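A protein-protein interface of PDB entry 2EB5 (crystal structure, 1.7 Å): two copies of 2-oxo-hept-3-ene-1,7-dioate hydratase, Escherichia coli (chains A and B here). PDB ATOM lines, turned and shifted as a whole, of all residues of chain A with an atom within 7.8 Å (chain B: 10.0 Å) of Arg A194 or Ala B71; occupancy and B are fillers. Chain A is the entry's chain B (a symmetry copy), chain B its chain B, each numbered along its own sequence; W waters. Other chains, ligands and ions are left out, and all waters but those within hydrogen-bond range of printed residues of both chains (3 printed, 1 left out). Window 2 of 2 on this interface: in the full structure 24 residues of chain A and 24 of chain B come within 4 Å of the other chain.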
ATOM      1  N   PRO A 103     -14.648  -8.469  19.719  1.00  0.00           N
ATOM      2  CA  PRO A 103     -13.718  -9.170  20.616  1.00  0.00           C
ATOM      3  C   PRO A 103     -14.096 -10.626  20.851  1.00  0.00           C
ATOM      4  O   PRO A 103     -15.282 -10.960  20.936  1.00  0.00           O
ATOM      5  CB  PRO A 103     -13.852  -8.393  21.935  1.00  0.00           C
ATOM      6  CG  PRO A 103     -15.264  -7.897  21.908  1.00  0.00           C
ATOM      7  CD  PRO A 103     -15.470  -7.489  20.452  1.00  0.00           C
ATOM      8  N   ILE A 105     -12.641 -14.247  23.222  1.00  0.00           N
ATOM      9  CA  ILE A 105     -11.793 -14.749  24.303  1.00  0.00           C
ATOM     10  C   ILE A 105     -11.245 -16.120  23.932  1.00  0.00           C
ATOM     11  O   ILE A 105     -11.984 -16.995  23.433  1.00  0.00           O
ATOM     12  CB  ILE A 105     -12.595 -14.876  25.673  1.00  0.00           C
ATOM     13  CG1 ILE A 105     -12.939 -13.503  26.235  1.00  0.00           C
ATOM     14  CG2 ILE A 105     -11.831 -15.743  26.681  1.00  0.00           C
ATOM     15  CD1 ILE A 105     -11.765 -12.776  26.966  1.00  0.00           C
ATOM     16  N   LEU A 191     -11.765 -25.435  31.195  1.00  0.00           N
ATOM     17  CA  LEU A 191     -13.151 -25.315  30.783  1.00  0.00           C
ATOM     18  C   LEU A 191     -13.448 -23.835  30.651  1.00  0.00           C
ATOM     19  O   LEU A 191     -13.309 -23.103  31.626  1.00  0.00           O
ATOM     20  CB  LEU A 191     -14.095 -25.883  31.859  1.00  0.00           C
ATOM     21  CG  LEU A 191     -13.676 -27.221  32.448  1.00  0.00           C
ATOM     22  CD1 LEU A 191     -14.559 -27.594  33.646  1.00  0.00           C
ATOM     23  CD2 LEU A 191     -13.680 -28.377  31.381  1.00  0.00           C
ATOM     24  N   MET A 192     -13.843 -23.398  29.453  1.00  0.00           N
ATOM     25  CA  MET A 192     -14.226 -21.999  29.268  1.00  0.00           C
ATOM     26  C   MET A 192     -15.735 -21.828  29.392  1.00  0.00           C
ATOM     27  O   MET A 192     -16.492 -22.260  28.512  1.00  0.00           O
ATOM     28  CB  MET A 192     -13.802 -21.421  27.920  1.00  0.00           C
ATOM     29  CG  MET A 192     -14.206 -19.926  27.868  1.00  0.00           C
ATOM     30  SD  MET A 192     -14.356 -19.290  26.212  1.00  0.00           S
ATOM     31  CE  MET A 192     -12.860 -19.836  25.366  1.00  0.00           C
ATOM     32  N   TYR A 193     -16.163 -21.193  30.475  1.00  0.00           N
ATOM     33  CA  TYR A 193     -17.581 -20.828  30.663  1.00  0.00           C
ATOM     34  C   TYR A 193     -17.810 -19.415  30.173  1.00  0.00           C
ATOM     35  O   TYR A 193     -16.948 -18.524  30.339  1.00  0.00           O
ATOM     36  CB  TYR A 193     -18.026 -20.847  32.142  1.00  0.00           C
ATOM     37  CG  TYR A 193     -17.931 -22.163  32.856  1.00  0.00           C
ATOM     38  CD1 TYR A 193     -19.099 -22.855  33.225  1.00  0.00           C
ATOM     39  CD2 TYR A 193     -16.682 -22.709  33.183  1.00  0.00           C
ATOM     40  CE1 TYR A 193     -19.036 -24.069  33.879  1.00  0.00           C
ATOM     41  CE2 TYR A 193     -16.600 -23.911  33.842  1.00  0.00           C
ATOM     42  CZ  TYR A 193     -17.795 -24.586  34.184  1.00  0.00           C
ATOM     43  OH  TYR A 193     -17.752 -25.790  34.831  1.00  0.00           O
ATOM     44  N   ARG A 194     -18.983 -19.211  29.571  1.00  0.00           N
ATOM     45  CA  ARG A 194     -19.481 -17.851  29.311  1.00  0.00           C
ATOM     46  C   ARG A 194     -20.933 -17.830  29.776  1.00  0.00           C
ATOM     47  O   ARG A 194     -21.717 -18.692  29.388  1.00  0.00           O
ATOM     48  CB  ARG A 194     -19.400 -17.511  27.819  1.00  0.00           C
ATOM     49  CG  ARG A 194     -19.910 -16.129  27.472  1.00  0.00           C
ATOM     50  CD  ARG A 194     -19.933 -15.940  25.930  1.00  0.00           C
ATOM     51  NE  ARG A 194     -20.878 -16.853  25.283  1.00  0.00           N
ATOM     52  CZ  ARG A 194     -21.097 -16.938  23.959  1.00  0.00           C
ATOM     53  NH1 ARG A 194     -20.430 -16.161  23.086  1.00  0.00           N
ATOM     54  NH2 ARG A 194     -21.979 -17.824  23.495  1.00  0.00           N
ATOM     55  N   ASN A 195     -21.281 -16.846  30.608  1.00  0.00           N
ATOM     56  CA  ASN A 195     -22.650 -16.773  31.125  1.00  0.00           C
ATOM     57  C   ASN A 195     -23.102 -18.085  31.747  1.00  0.00           C
ATOM     58  O   ASN A 195     -24.261 -18.468  31.648  1.00  0.00           O
ATOM     59  CB  ASN A 195     -23.625 -16.304  30.036  1.00  0.00           C
ATOM     60  CG  ASN A 195     -23.270 -14.958  29.524  1.00  0.00           C
ATOM     61  OD1 ASN A 195     -22.737 -14.148  30.265  1.00  0.00           O
ATOM     62  ND2 ASN A 195     -23.494 -14.726  28.232  1.00  0.00           N
ATOM     63  N   GLY A 196     -22.174 -18.755  32.426  1.00  0.00           N
ATOM     64  CA  GLY A 196     -22.545 -19.928  33.238  1.00  0.00           C
ATOM     65  C   GLY A 196     -22.569 -21.259  32.518  1.00  0.00           C
ATOM     66  O   GLY A 196     -22.856 -22.286  33.128  1.00  0.00           O
ATOM     67  N   VAL A 197     -22.236 -21.239  31.232  1.00  0.00           N
ATOM     68  CA  VAL A 197     -22.290 -22.401  30.381  1.00  0.00           C
ATOM     69  C   VAL A 197     -20.924 -22.662  29.766  1.00  0.00           C
ATOM     70  O   VAL A 197     -20.275 -21.747  29.302  1.00  0.00           O
ATOM     71  CB  VAL A 197     -23.349 -22.132  29.253  1.00  0.00           C
ATOM     72  CG1 VAL A 197     -23.204 -23.076  28.067  1.00  0.00           C
ATOM     73  CG2 VAL A 197     -24.757 -22.207  29.886  1.00  0.00           C
ATOM     74  N   ILE A 198     -20.501 -23.920  29.719  1.00  0.00           N
ATOM     75  CA  ILE A 198     -19.212 -24.259  29.110  1.00  0.00           C
ATOM     76  C   ILE A 198     -19.361 -24.192  27.597  1.00  0.00           C
ATOM     77  O   ILE A 198     -20.161 -24.943  27.003  1.00  0.00           O
ATOM     78  CB  ILE A 198     -18.751 -25.682  29.515  1.00  0.00           C
ATOM     79  CG1 ILE A 198     -18.465 -25.745  31.021  1.00  0.00           C
ATOM     80  CG2 ILE A 198     -17.534 -26.123  28.694  1.00  0.00           C
ATOM     81  CD1 ILE A 198     -18.258 -27.203  31.518  1.00  0.00           C
ATOM     82  N   GLU A 199     -18.586 -23.302  26.996  1.00  0.00           N
ATOM     83  CA  GLU A 199     -18.589 -23.086  25.539  1.00  0.00           C
ATOM     84  C   GLU A 199     -17.488 -23.837  24.825  1.00  0.00           C
ATOM     85  O   GLU A 199     -17.672 -24.238  23.658  1.00  0.00           O
ATOM     86  CB  GLU A 199     -18.491 -21.596  25.209  1.00  0.00           C
ATOM     87  CG  GLU A 199     -19.788 -20.833  25.545  1.00  0.00           C
ATOM     88  CD  GLU A 199     -20.941 -21.101  24.586  1.00  0.00           C
ATOM     89  OE1 GLU A 199     -20.747 -21.728  23.518  1.00  0.00           O
ATOM     90  OE2 GLU A 199     -22.048 -20.654  24.909  1.00  0.00           O
ATOM     91  N   GLU A 200     -16.343 -24.005  25.488  1.00  0.00           N
ATOM     92  CA  GLU A 200     -15.193 -24.741  24.914  1.00  0.00           C
ATOM     93  C   GLU A 200     -14.439 -25.416  26.025  1.00  0.00           C
ATOM     94  O   GLU A 200     -14.408 -24.912  27.154  1.00  0.00           O
ATOM     95  CB  GLU A 200     -14.198 -23.811  24.183  1.00  0.00           C
ATOM     96  CG  GLU A 200     -14.750 -23.071  22.930  1.00  0.00           C
ATOM     97  CD  GLU A 200     -15.114 -23.994  21.771  1.00  0.00           C
ATOM     98  OE1 GLU A 200     -14.601 -25.133  21.695  1.00  0.00           O
ATOM     99  OE2 GLU A 200     -15.936 -23.574  20.913  1.00  0.00           O
ATOM    100  N   PRO A 243     -11.736 -19.468  19.781  1.00  0.00           N
ATOM    101  CA  PRO A 243     -12.118 -18.224  20.446  1.00  0.00           C
ATOM    102  C   PRO A 243     -13.624 -18.146  20.569  1.00  0.00           C
ATOM    103  O   PRO A 243     -14.345 -18.697  19.705  1.00  0.00           O
ATOM    104  CB  PRO A 243     -11.634 -17.112  19.485  1.00  0.00           C
ATOM    105  CG  PRO A 243     -10.816 -17.779  18.452  1.00  0.00           C
ATOM    106  CD  PRO A 243     -11.249 -19.233  18.411  1.00  0.00           C
ATOM    107  N   VAL A 244     -14.103 -17.468  21.609  1.00  0.00           N
ATOM    108  CA  VAL A 244     -15.540 -17.334  21.855  1.00  0.00           C
ATOM    109  C   VAL A 244     -15.927 -15.845  21.883  1.00  0.00           C
ATOM    110  O   VAL A 244     -15.280 -15.073  22.595  1.00  0.00           O
ATOM    111  CB  VAL A 244     -15.940 -18.039  23.188  1.00  0.00           C
ATOM    112  CG1 VAL A 244     -17.378 -17.702  23.603  1.00  0.00           C
ATOM    113  CG2 VAL A 244     -15.756 -19.567  23.037  1.00  0.00           C
ATOM    114  N   PRO A 245     -16.938 -15.440  21.078  1.00  0.00           N
ATOM    115  CA  PRO A 245     -17.300 -14.019  21.086  1.00  0.00           C
ATOM    116  C   PRO A 245     -17.656 -13.478  22.474  1.00  0.00           C
ATOM    117  O   PRO A 245     -18.359 -14.135  23.279  1.00  0.00           O
ATOM    118  CB  PRO A 245     -18.507 -13.944  20.131  1.00  0.00           C
ATOM    119  CG  PRO A 245     -18.283 -15.117  19.183  1.00  0.00           C
ATOM    120  CD  PRO A 245     -17.739 -16.205  20.102  1.00  0.00           C
ATOM    121  N   ALA A 246     -17.186 -12.265  22.708  1.00  0.00           N
ATOM    122  CA  ALA A 246     -17.475 -11.510  23.929  1.00  0.00           C
ATOM    123  C   ALA A 246     -18.423 -10.367  23.589  1.00  0.00           C
ATOM    124  O   ALA A 246     -18.128  -9.558  22.698  1.00  0.00           O
ATOM    125  CB  ALA A 246     -16.196 -10.967  24.479  1.00  0.00           C
ATOM    126  N   ARG A 247     -19.563 -10.309  24.277  1.00  0.00           N
ATOM    127  CA  ARG A 247     -20.574  -9.282  24.051  1.00  0.00           C
ATOM    128  C   ARG A 247     -20.805  -8.553  25.355  1.00  0.00           C
ATOM    129  O   ARG A 247     -20.573  -9.112  26.438  1.00  0.00           O
ATOM    130  CB  ARG A 247     -21.893  -9.900  23.585  1.00  0.00           C
ATOM    131  CG  ARG A 247     -21.861 -10.549  22.205  1.00  0.00           C
ATOM    132  CD  ARG A 247     -21.396 -12.013  22.232  1.00  0.00           C
ATOM    133  NE  ARG A 247     -21.922 -12.761  23.384  1.00  0.00           N
ATOM    134  CZ  ARG A 247     -22.944 -13.604  23.339  1.00  0.00           C
ATOM    135  NH1 ARG A 247     -23.340 -14.232  24.435  1.00  0.00           N
ATOM    136  NH2 ARG A 247     -23.565 -13.834  22.186  1.00  0.00           N
ATOM    137  N   GLY A 249     -22.202  -7.430  28.666  1.00  0.00           N
ATOM    138  CA  GLY A 249     -23.025  -8.206  29.584  1.00  0.00           C
ATOM    139  C   GLY A 249     -22.534  -9.626  29.822  1.00  0.00           C
ATOM    140  O   GLY A 249     -23.019 -10.315  30.717  1.00  0.00           O
ATOM    141  N   ASP A 250     -21.567 -10.078  29.035  1.00  0.00           N
ATOM    142  CA  ASP A 250     -21.102 -11.458  29.166  1.00  0.00           C
ATOM    143  C   ASP A 250     -20.125 -11.555  30.327  1.00  0.00           C
ATOM    144  O   ASP A 250     -19.258 -10.706  30.461  1.00  0.00           O
ATOM    145  CB  ASP A 250     -20.343 -11.896  27.913  1.00  0.00           C
ATOM    146  CG  ASP A 250     -21.254 -12.279  26.754  1.00  0.00           C
ATOM    147  OD1 ASP A 250     -22.489 -12.428  26.914  1.00  0.00           O
ATOM    148  OD2 ASP A 250     -20.671 -12.473  25.667  1.00  0.00           O
ATOM    149  N   THR A 251     -20.248 -12.616  31.127  1.00  0.00           N
ATOM    150  CA  THR A 251     -19.227 -12.972  32.115  1.00  0.00           C
ATOM    151  C   THR A 251     -18.495 -14.199  31.554  1.00  0.00           C
ATOM    152  O   THR A 251     -19.148 -15.096  31.042  1.00  0.00           O
ATOM    153  CB  THR A 251     -19.852 -13.359  33.470  1.00  0.00           C
ATOM    154  OG1 THR A 251     -20.599 -12.248  33.980  1.00  0.00           O
ATOM    155  CG2 THR A 251     -18.774 -13.704  34.470  1.00  0.00           C
ATOM    156  N   PHE A 252     -17.173 -14.214  31.641  1.00  0.00           N
ATOM    157  CA  PHE A 252     -16.383 -15.424  31.334  1.00  0.00           C
ATOM    158  C   PHE A 252     -15.745 -15.921  32.622  1.00  0.00           C
ATOM    159  O   PHE A 252     -15.387 -15.114  33.471  1.00  0.00           O
ATOM    160  CB  PHE A 252     -15.276 -15.095  30.344  1.00  0.00           C
ATOM    161  CG  PHE A 252     -15.783 -14.874  28.931  1.00  0.00           C
ATOM    162  CD1 PHE A 252     -15.669 -15.873  27.962  1.00  0.00           C
ATOM    163  CD2 PHE A 252     -16.368 -13.655  28.587  1.00  0.00           C
ATOM    164  CE1 PHE A 252     -16.184 -15.649  26.652  1.00  0.00           C
ATOM    165  CE2 PHE A 252     -16.837 -13.415  27.313  1.00  0.00           C
ATOM    166  CZ  PHE A 252     -16.763 -14.393  26.338  1.00  0.00           C
ATOM    167  N   HIS A 253     -15.589 -17.243  32.733  1.00  0.00           N
ATOM    168  CA  HIS A 253     -14.886 -17.857  33.843  1.00  0.00           C
ATOM    169  C   HIS A 253     -14.193 -19.064  33.269  1.00  0.00           C
ATOM    170  O   HIS A 253     -14.836 -19.978  32.796  1.00  0.00           O
ATOM    171  CB  HIS A 253     -15.859 -18.334  34.905  1.00  0.00           C
ATOM    172  CG  HIS A 253     -15.185 -18.905  36.122  1.00  0.00           C
ATOM    173  ND1 HIS A 253     -15.130 -18.229  37.325  1.00  0.00           N
ATOM    174  CD2 HIS A 253     -14.511 -20.062  36.307  1.00  0.00           C
ATOM    175  CE1 HIS A 253     -14.455 -18.950  38.202  1.00  0.00           C
ATOM    176  NE2 HIS A 253     -14.064 -20.069  37.610  1.00  0.00           N
ATOM    177  N   VAL A 254     -12.875 -19.077  33.343  1.00  0.00           N
ATOM    178  CA  VAL A 254     -12.117 -20.133  32.676  1.00  0.00           C
ATOM    179  C   VAL A 254     -11.438 -20.906  33.789  1.00  0.00           C
ATOM    180  O   VAL A 254     -10.598 -20.369  34.517  1.00  0.00           O
ATOM    181  CB  VAL A 254     -11.107 -19.589  31.645  1.00  0.00           C
ATOM    182  CG1 VAL A 254     -10.353 -20.756  30.994  1.00  0.00           C
ATOM    183  CG2 VAL A 254     -11.835 -18.740  30.557  1.00  0.00           C
ATOM    184  N   PHE A 266     -17.679  -8.326  30.625  1.00  0.00           N
ATOM    185  CA  PHE A 266     -17.733  -7.264  29.619  1.00  0.00           C
ATOM    186  C   PHE A 266     -18.870  -6.305  29.942  1.00  0.00           C
ATOM    187  O   PHE A 266     -20.015  -6.724  30.088  1.00  0.00           O
ATOM    188  CB  PHE A 266     -17.901  -7.879  28.238  1.00  0.00           C
ATOM    189  CG  PHE A 266     -16.639  -8.476  27.745  1.00  0.00           C
ATOM    190  CD1 PHE A 266     -15.807  -7.751  26.900  1.00  0.00           C
ATOM    191  CD2 PHE A 266     -16.217  -9.749  28.208  1.00  0.00           C
ATOM    192  CE1 PHE A 266     -14.576  -8.294  26.484  1.00  0.00           C
ATOM    193  CE2 PHE A 266     -15.014 -10.291  27.810  1.00  0.00           C
ATOM    194  CZ  PHE A 266     -14.182  -9.566  26.936  1.00  0.00           C
ATOM    195  N   THR B  65     -24.677 -32.960  22.463  1.00  0.00           N
ATOM    196  CA  THR B  65     -24.533 -32.429  23.813  1.00  0.00           C
ATOM    197  C   THR B  65     -23.861 -31.051  23.761  1.00  0.00           C
ATOM    198  O   THR B  65     -24.344 -30.099  24.375  1.00  0.00           O
ATOM    199  CB  THR B  65     -23.748 -33.405  24.692  1.00  0.00           C
ATOM    200  OG1 THR B  65     -22.524 -33.733  24.029  1.00  0.00           O
ATOM    201  CG2 THR B  65     -24.532 -34.676  24.896  1.00  0.00           C
ATOM    202  N   SER B  66     -22.781 -30.925  22.993  1.00  0.00           N
ATOM    203  CA  SER B  66     -22.102 -29.626  22.839  1.00  0.00           C
ATOM    204  C   SER B  66     -23.073 -28.584  22.300  1.00  0.00           C
ATOM    205  O   SER B  66     -23.208 -27.499  22.882  1.00  0.00           O
ATOM    206  CB  SER B  66     -20.881 -29.753  21.934  1.00  0.00           C
ATOM    207  OG  SER B  66     -19.934 -30.643  22.531  1.00  0.00           O
ATOM    208  N   LYS B  67     -23.784 -28.929  21.219  1.00  0.00           N
ATOM    209  CA  LYS B  67     -24.753 -28.008  20.588  1.00  0.00           C
ATOM    210  C   LYS B  67     -25.940 -27.680  21.492  1.00  0.00           C
ATOM    211  O   LYS B  67     -26.391 -26.540  21.521  1.00  0.00           O
ATOM    212  CB  LYS B  67     -25.195 -28.507  19.208  1.00  0.00           C
ATOM    213  CG  LYS B  67     -24.069 -28.420  18.187  1.00  0.00           C
ATOM    214  CD  LYS B  67     -23.939 -29.701  17.383  1.00  0.00           C
ATOM    215  CE  LYS B  67     -24.533 -29.562  15.981  1.00  0.00           C
ATOM    216  NZ  LYS B  67     -23.772 -28.563  15.158  1.00  0.00           N
ATOM    217  N   ALA B  68     -26.423 -28.655  22.258  1.00  0.00           N
ATOM    218  CA  ALA B  68     -27.463 -28.365  23.244  1.00  0.00           C
ATOM    219  C   ALA B  68     -26.979 -27.288  24.232  1.00  0.00           C
ATOM    220  O   ALA B  68     -27.754 -26.410  24.623  1.00  0.00           O
ATOM    221  CB  ALA B  68     -27.898 -29.623  23.971  1.00  0.00           C
ATOM    222  N   MET B  69     -25.691 -27.334  24.592  1.00  0.00           N
ATOM    223  CA  MET B  69     -25.095 -26.370  25.548  1.00  0.00           C
ATOM    224  C   MET B  69     -24.670 -25.024  24.943  1.00  0.00           C
ATOM    225  O   MET B  69     -24.832 -23.985  25.581  1.00  0.00           O
ATOM    226  CB  MET B  69     -23.880 -26.970  26.253  1.00  0.00           C
ATOM    227  CG  MET B  69     -24.135 -28.256  26.995  1.00  0.00           C
ATOM    228  SD  MET B  69     -22.563 -29.088  27.197  1.00  0.00           S
ATOM    229  CE  MET B  69     -21.839 -28.189  28.593  1.00  0.00           C
ATOM    230  N   GLN B  70     -24.085 -25.054  23.744  1.00  0.00           N
ATOM    231  CA  GLN B  70     -23.637 -23.837  23.064  1.00  0.00           C
ATOM    232  C   GLN B  70     -24.780 -22.842  22.840  1.00  0.00           C
ATOM    233  O   GLN B  70     -25.818 -23.195  22.266  1.00  0.00           O
ATOM    234  CB  GLN B  70     -23.012 -24.180  21.722  1.00  0.00           C
ATOM    235  CG  GLN B  70     -21.659 -24.869  21.816  1.00  0.00           C
ATOM    236  CD  GLN B  70     -21.336 -25.646  20.546  1.00  0.00           C
ATOM    237  OE1 GLN B  70     -20.475 -26.534  20.546  1.00  0.00           O
ATOM    238  NE2 GLN B  70     -22.049 -25.332  19.460  1.00  0.00           N
ATOM    239  N   ALA B  71     -24.577 -21.604  23.296  1.00  0.00           N
ATOM    240  CA  ALA B  71     -25.575 -20.543  23.152  1.00  0.00           C
ATOM    241  C   ALA B  71     -25.832 -20.169  21.677  1.00  0.00           C
ATOM    242  O   ALA B  71     -26.947 -19.787  21.314  1.00  0.00           O
ATOM    243  CB  ALA B  71     -25.172 -19.314  23.974  1.00  0.00           C
ATOM    244  N   SER B  72     -24.811 -20.307  20.834  1.00  0.00           N
ATOM    245  CA  SER B  72     -24.921 -19.980  19.401  1.00  0.00           C
ATOM    246  C   SER B  72     -25.697 -21.016  18.580  1.00  0.00           C
ATOM    247  O   SER B  72     -25.892 -20.834  17.372  1.00  0.00           O
ATOM    248  CB  SER B  72     -23.527 -19.811  18.779  1.00  0.00           C
ATOM    249  OG  SER B  72     -22.848 -21.062  18.704  1.00  0.00           O
ATOM    250  N   SER B  73     -26.107 -22.108  19.222  1.00  0.00           N
ATOM    251  CA  SER B  73     -26.823 -23.185  18.545  1.00  0.00           C
ATOM    252  C   SER B  73     -28.274 -23.203  18.976  1.00  0.00           C
ATOM    253  O   SER B  73     -28.579 -23.103  20.172  1.00  0.00           O
ATOM    254  CB  SER B  73     -26.172 -24.546  18.834  1.00  0.00           C
ATOM    255  OG  SER B  73     -27.042 -25.611  18.486  1.00  0.00           O
ATOM    256  N   GLN B  74     -29.162 -23.345  17.997  1.00  0.00           N
ATOM    257  CA  GLN B  74     -30.604 -23.403  18.258  1.00  0.00           C
ATOM    258  C   GLN B  74     -31.091 -24.724  18.912  1.00  0.00           C
ATOM    259  O   GLN B  74     -32.228 -24.788  19.408  1.00  0.00           O
ATOM    260  CB  GLN B  74     -31.394 -23.073  16.980  1.00  0.00           C
ATOM    261  CG  GLN B  74     -31.185 -21.624  16.468  1.00  0.00           C
ATOM    262  CD  GLN B  74     -32.179 -21.232  15.370  1.00  0.00           C
ATOM    263  OE1 GLN B  74     -32.046 -21.650  14.214  1.00  0.00           O
ATOM    264  NE2 GLN B  74     -33.179 -20.423  15.733  1.00  0.00           N
ATOM    265  N   ILE B  75     -30.238 -25.758  18.917  1.00  0.00           N
ATOM    266  CA  ILE B  75     -30.550 -27.031  19.588  1.00  0.00           C
ATOM    267  C   ILE B  75     -30.765 -26.784  21.082  1.00  0.00           C
ATOM    268  O   ILE B  75     -29.892 -26.217  21.756  1.00  0.00           O
ATOM    269  CB  ILE B  75     -29.417 -28.095  19.454  1.00  0.00           C
ATOM    270  CG1 ILE B  75     -28.796 -28.131  18.042  1.00  0.00           C
ATOM    271  CG2 ILE B  75     -29.912 -29.473  19.959  1.00  0.00           C
ATOM    272  CD1 ILE B  75     -29.511 -29.009  17.009  1.00  0.00           C
ATOM    273  N   SER B  76     -31.920 -27.212  21.592  1.00  0.00           N
ATOM    274  CA  SER B  76     -32.283 -26.983  22.993  1.00  0.00           C
ATOM    275  C   SER B  76     -31.987 -28.154  23.921  1.00  0.00           C
ATOM    276  O   SER B  76     -31.952 -27.975  25.132  1.00  0.00           O
ATOM    277  CB  SER B  76     -33.764 -26.624  23.111  1.00  0.00           C
ATOM    278  OG  SER B  76     -34.570 -27.777  22.904  1.00  0.00           O
ATOM    279  N   ASN B 209     -21.873 -30.591  31.532  1.00  0.00           N
ATOM    280  CA  ASN B 209     -21.319 -30.289  32.868  1.00  0.00           C
ATOM    281  C   ASN B 209     -20.897 -31.513  33.706  1.00  0.00           C
ATOM    282  O   ASN B 209     -20.189 -31.385  34.700  1.00  0.00           O
ATOM    283  CB  ASN B 209     -22.332 -29.493  33.707  1.00  0.00           C
ATOM    284  CG  ASN B 209     -22.736 -28.194  33.063  1.00  0.00           C
ATOM    285  OD1 ASN B 209     -21.886 -27.353  32.758  1.00  0.00           O
ATOM    286  ND2 ASN B 209     -24.050 -28.008  32.864  1.00  0.00           N
ATOM    287  N   ARG B 242     -15.180 -31.808  18.861  1.00  0.00           N
ATOM    288  CA  ARG B 242     -15.836 -31.781  17.571  1.00  0.00           C
ATOM    289  C   ARG B 242     -15.386 -33.028  16.794  1.00  0.00           C
ATOM    290  O   ARG B 242     -14.296 -33.539  17.039  1.00  0.00           O
ATOM    291  CB  ARG B 242     -15.467 -30.531  16.810  1.00  0.00           C
ATOM    292  CG  ARG B 242     -16.045 -29.278  17.472  1.00  0.00           C
ATOM    293  CD  ARG B 242     -15.410 -28.042  16.848  1.00  0.00           C
ATOM    294  NE  ARG B 242     -16.101 -26.829  17.276  1.00  0.00           N
ATOM    295  CZ  ARG B 242     -15.911 -26.214  18.447  1.00  0.00           C
ATOM    296  NH1 ARG B 242     -15.032 -26.698  19.335  1.00  0.00           N
ATOM    297  NH2 ARG B 242     -16.593 -25.098  18.722  1.00  0.00           N
HETATM  298  O   HOH W   1     -22.443 -25.899  30.807  1.00  0.00           O
HETATM  299  O   HOH W   2     -20.057 -27.491  34.846  1.00  0.00           O
HETATM  300  O   HOH W   3     -19.823 -27.605  25.830  1.00  0.00           O
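The backbone NH of Ala B71 lies within hydrogen-bond range of the side-chain carboxylate of Glu A199 (3.1 Å).
The side-chain carboxylate (OE2) of Glu A200 is in salt-bridge range of the guanidinium group (NH2) of Arg B242, at 2.7 Å.
Ala B71 touches Arg A194.
Val A197 touches Met B69 (CG1 to O, 3.1 Å).
Ile A198 touches Met B69 (O to CE, 3.99 Å).
CD1 of Ile A198 touches OD1 of Asn B209 (3.8 Å).
OE1 of Glu A199 touches CA of Gln B70, 3.6 Å away.
O of Met A192 sits at hydrogen-bond distance from N of Glu A199, at 2.8 Å.
NH1 of Arg A194 sits at hydrogen-bond distance from O of Pro A245, 2.9 Å away.
The backbone NH (N) of Met A192 is in hydrogen-bond range of the backbone carbonyl oxygen (O) of Glu A200 (2.8 Å).
The guanidinium group (NH2) of Arg A194 lies within salt-bridge range of the side-chain carboxylate (OE2) of Glu A199 (3.2 Å).
Water W1 lies within hydrogen-bond range of OD1 of Asn B209 and N of Ile A198.
Water W2 bridges OD1 of Asn B209 (2.8 Å) and OH of Tyr A193 (2.9 Å).
Water W3 lies within hydrogen-bond range of O of Ile A198 (2.9 Å) and SD of Met B69 (3.4 Å).
Of the printed residues of chain B, Arg A194 touches Ala B71 (3.6 Å).
Ala B71 touches just these residues of chain A: Arg A194 and Glu A199.
No residue of chain B comes within 4 Å of Asn A195.
Val A197 touches just one residue of chain B: Met B69.
No residue of chain B comes within 4 Å of Pro A245.
Printed residues of chain B within 4 Å of Glu A199: Gln B70 (3.6 Å) and Ala B71 (3.1 Å).
Of the printed residues of chain A, Met B69 touches Val A197 and Ile A198.
Of the printed residues of chain A, Arg B242 touches Glu A200.
The nearest residue of chain A that does not touch Ala B71 is Val A197 (5.2 Å).
The nearest printed residue of chain B that does not touch Glu A199 is Met B69 (4.4 Å).
Of the 24 printed residues of chain A, 5 touch a printed residue of chain B.
Hydrophobic or aromatic side chains of chain A within 4 Å of the printed part of chain B: Val A197 and Ile A198.
Hydrophobic or aromatic side chains of chain B within 4 Å of the printed part of chain A: Met B69 and Ala B71.
Among the printed residues, 7 pairs touch across the chains.
No position is printed for both chains.
Of the 7 pairs that touch across the chains among the printed residues, none has its exchanged pair printed and touching as well.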
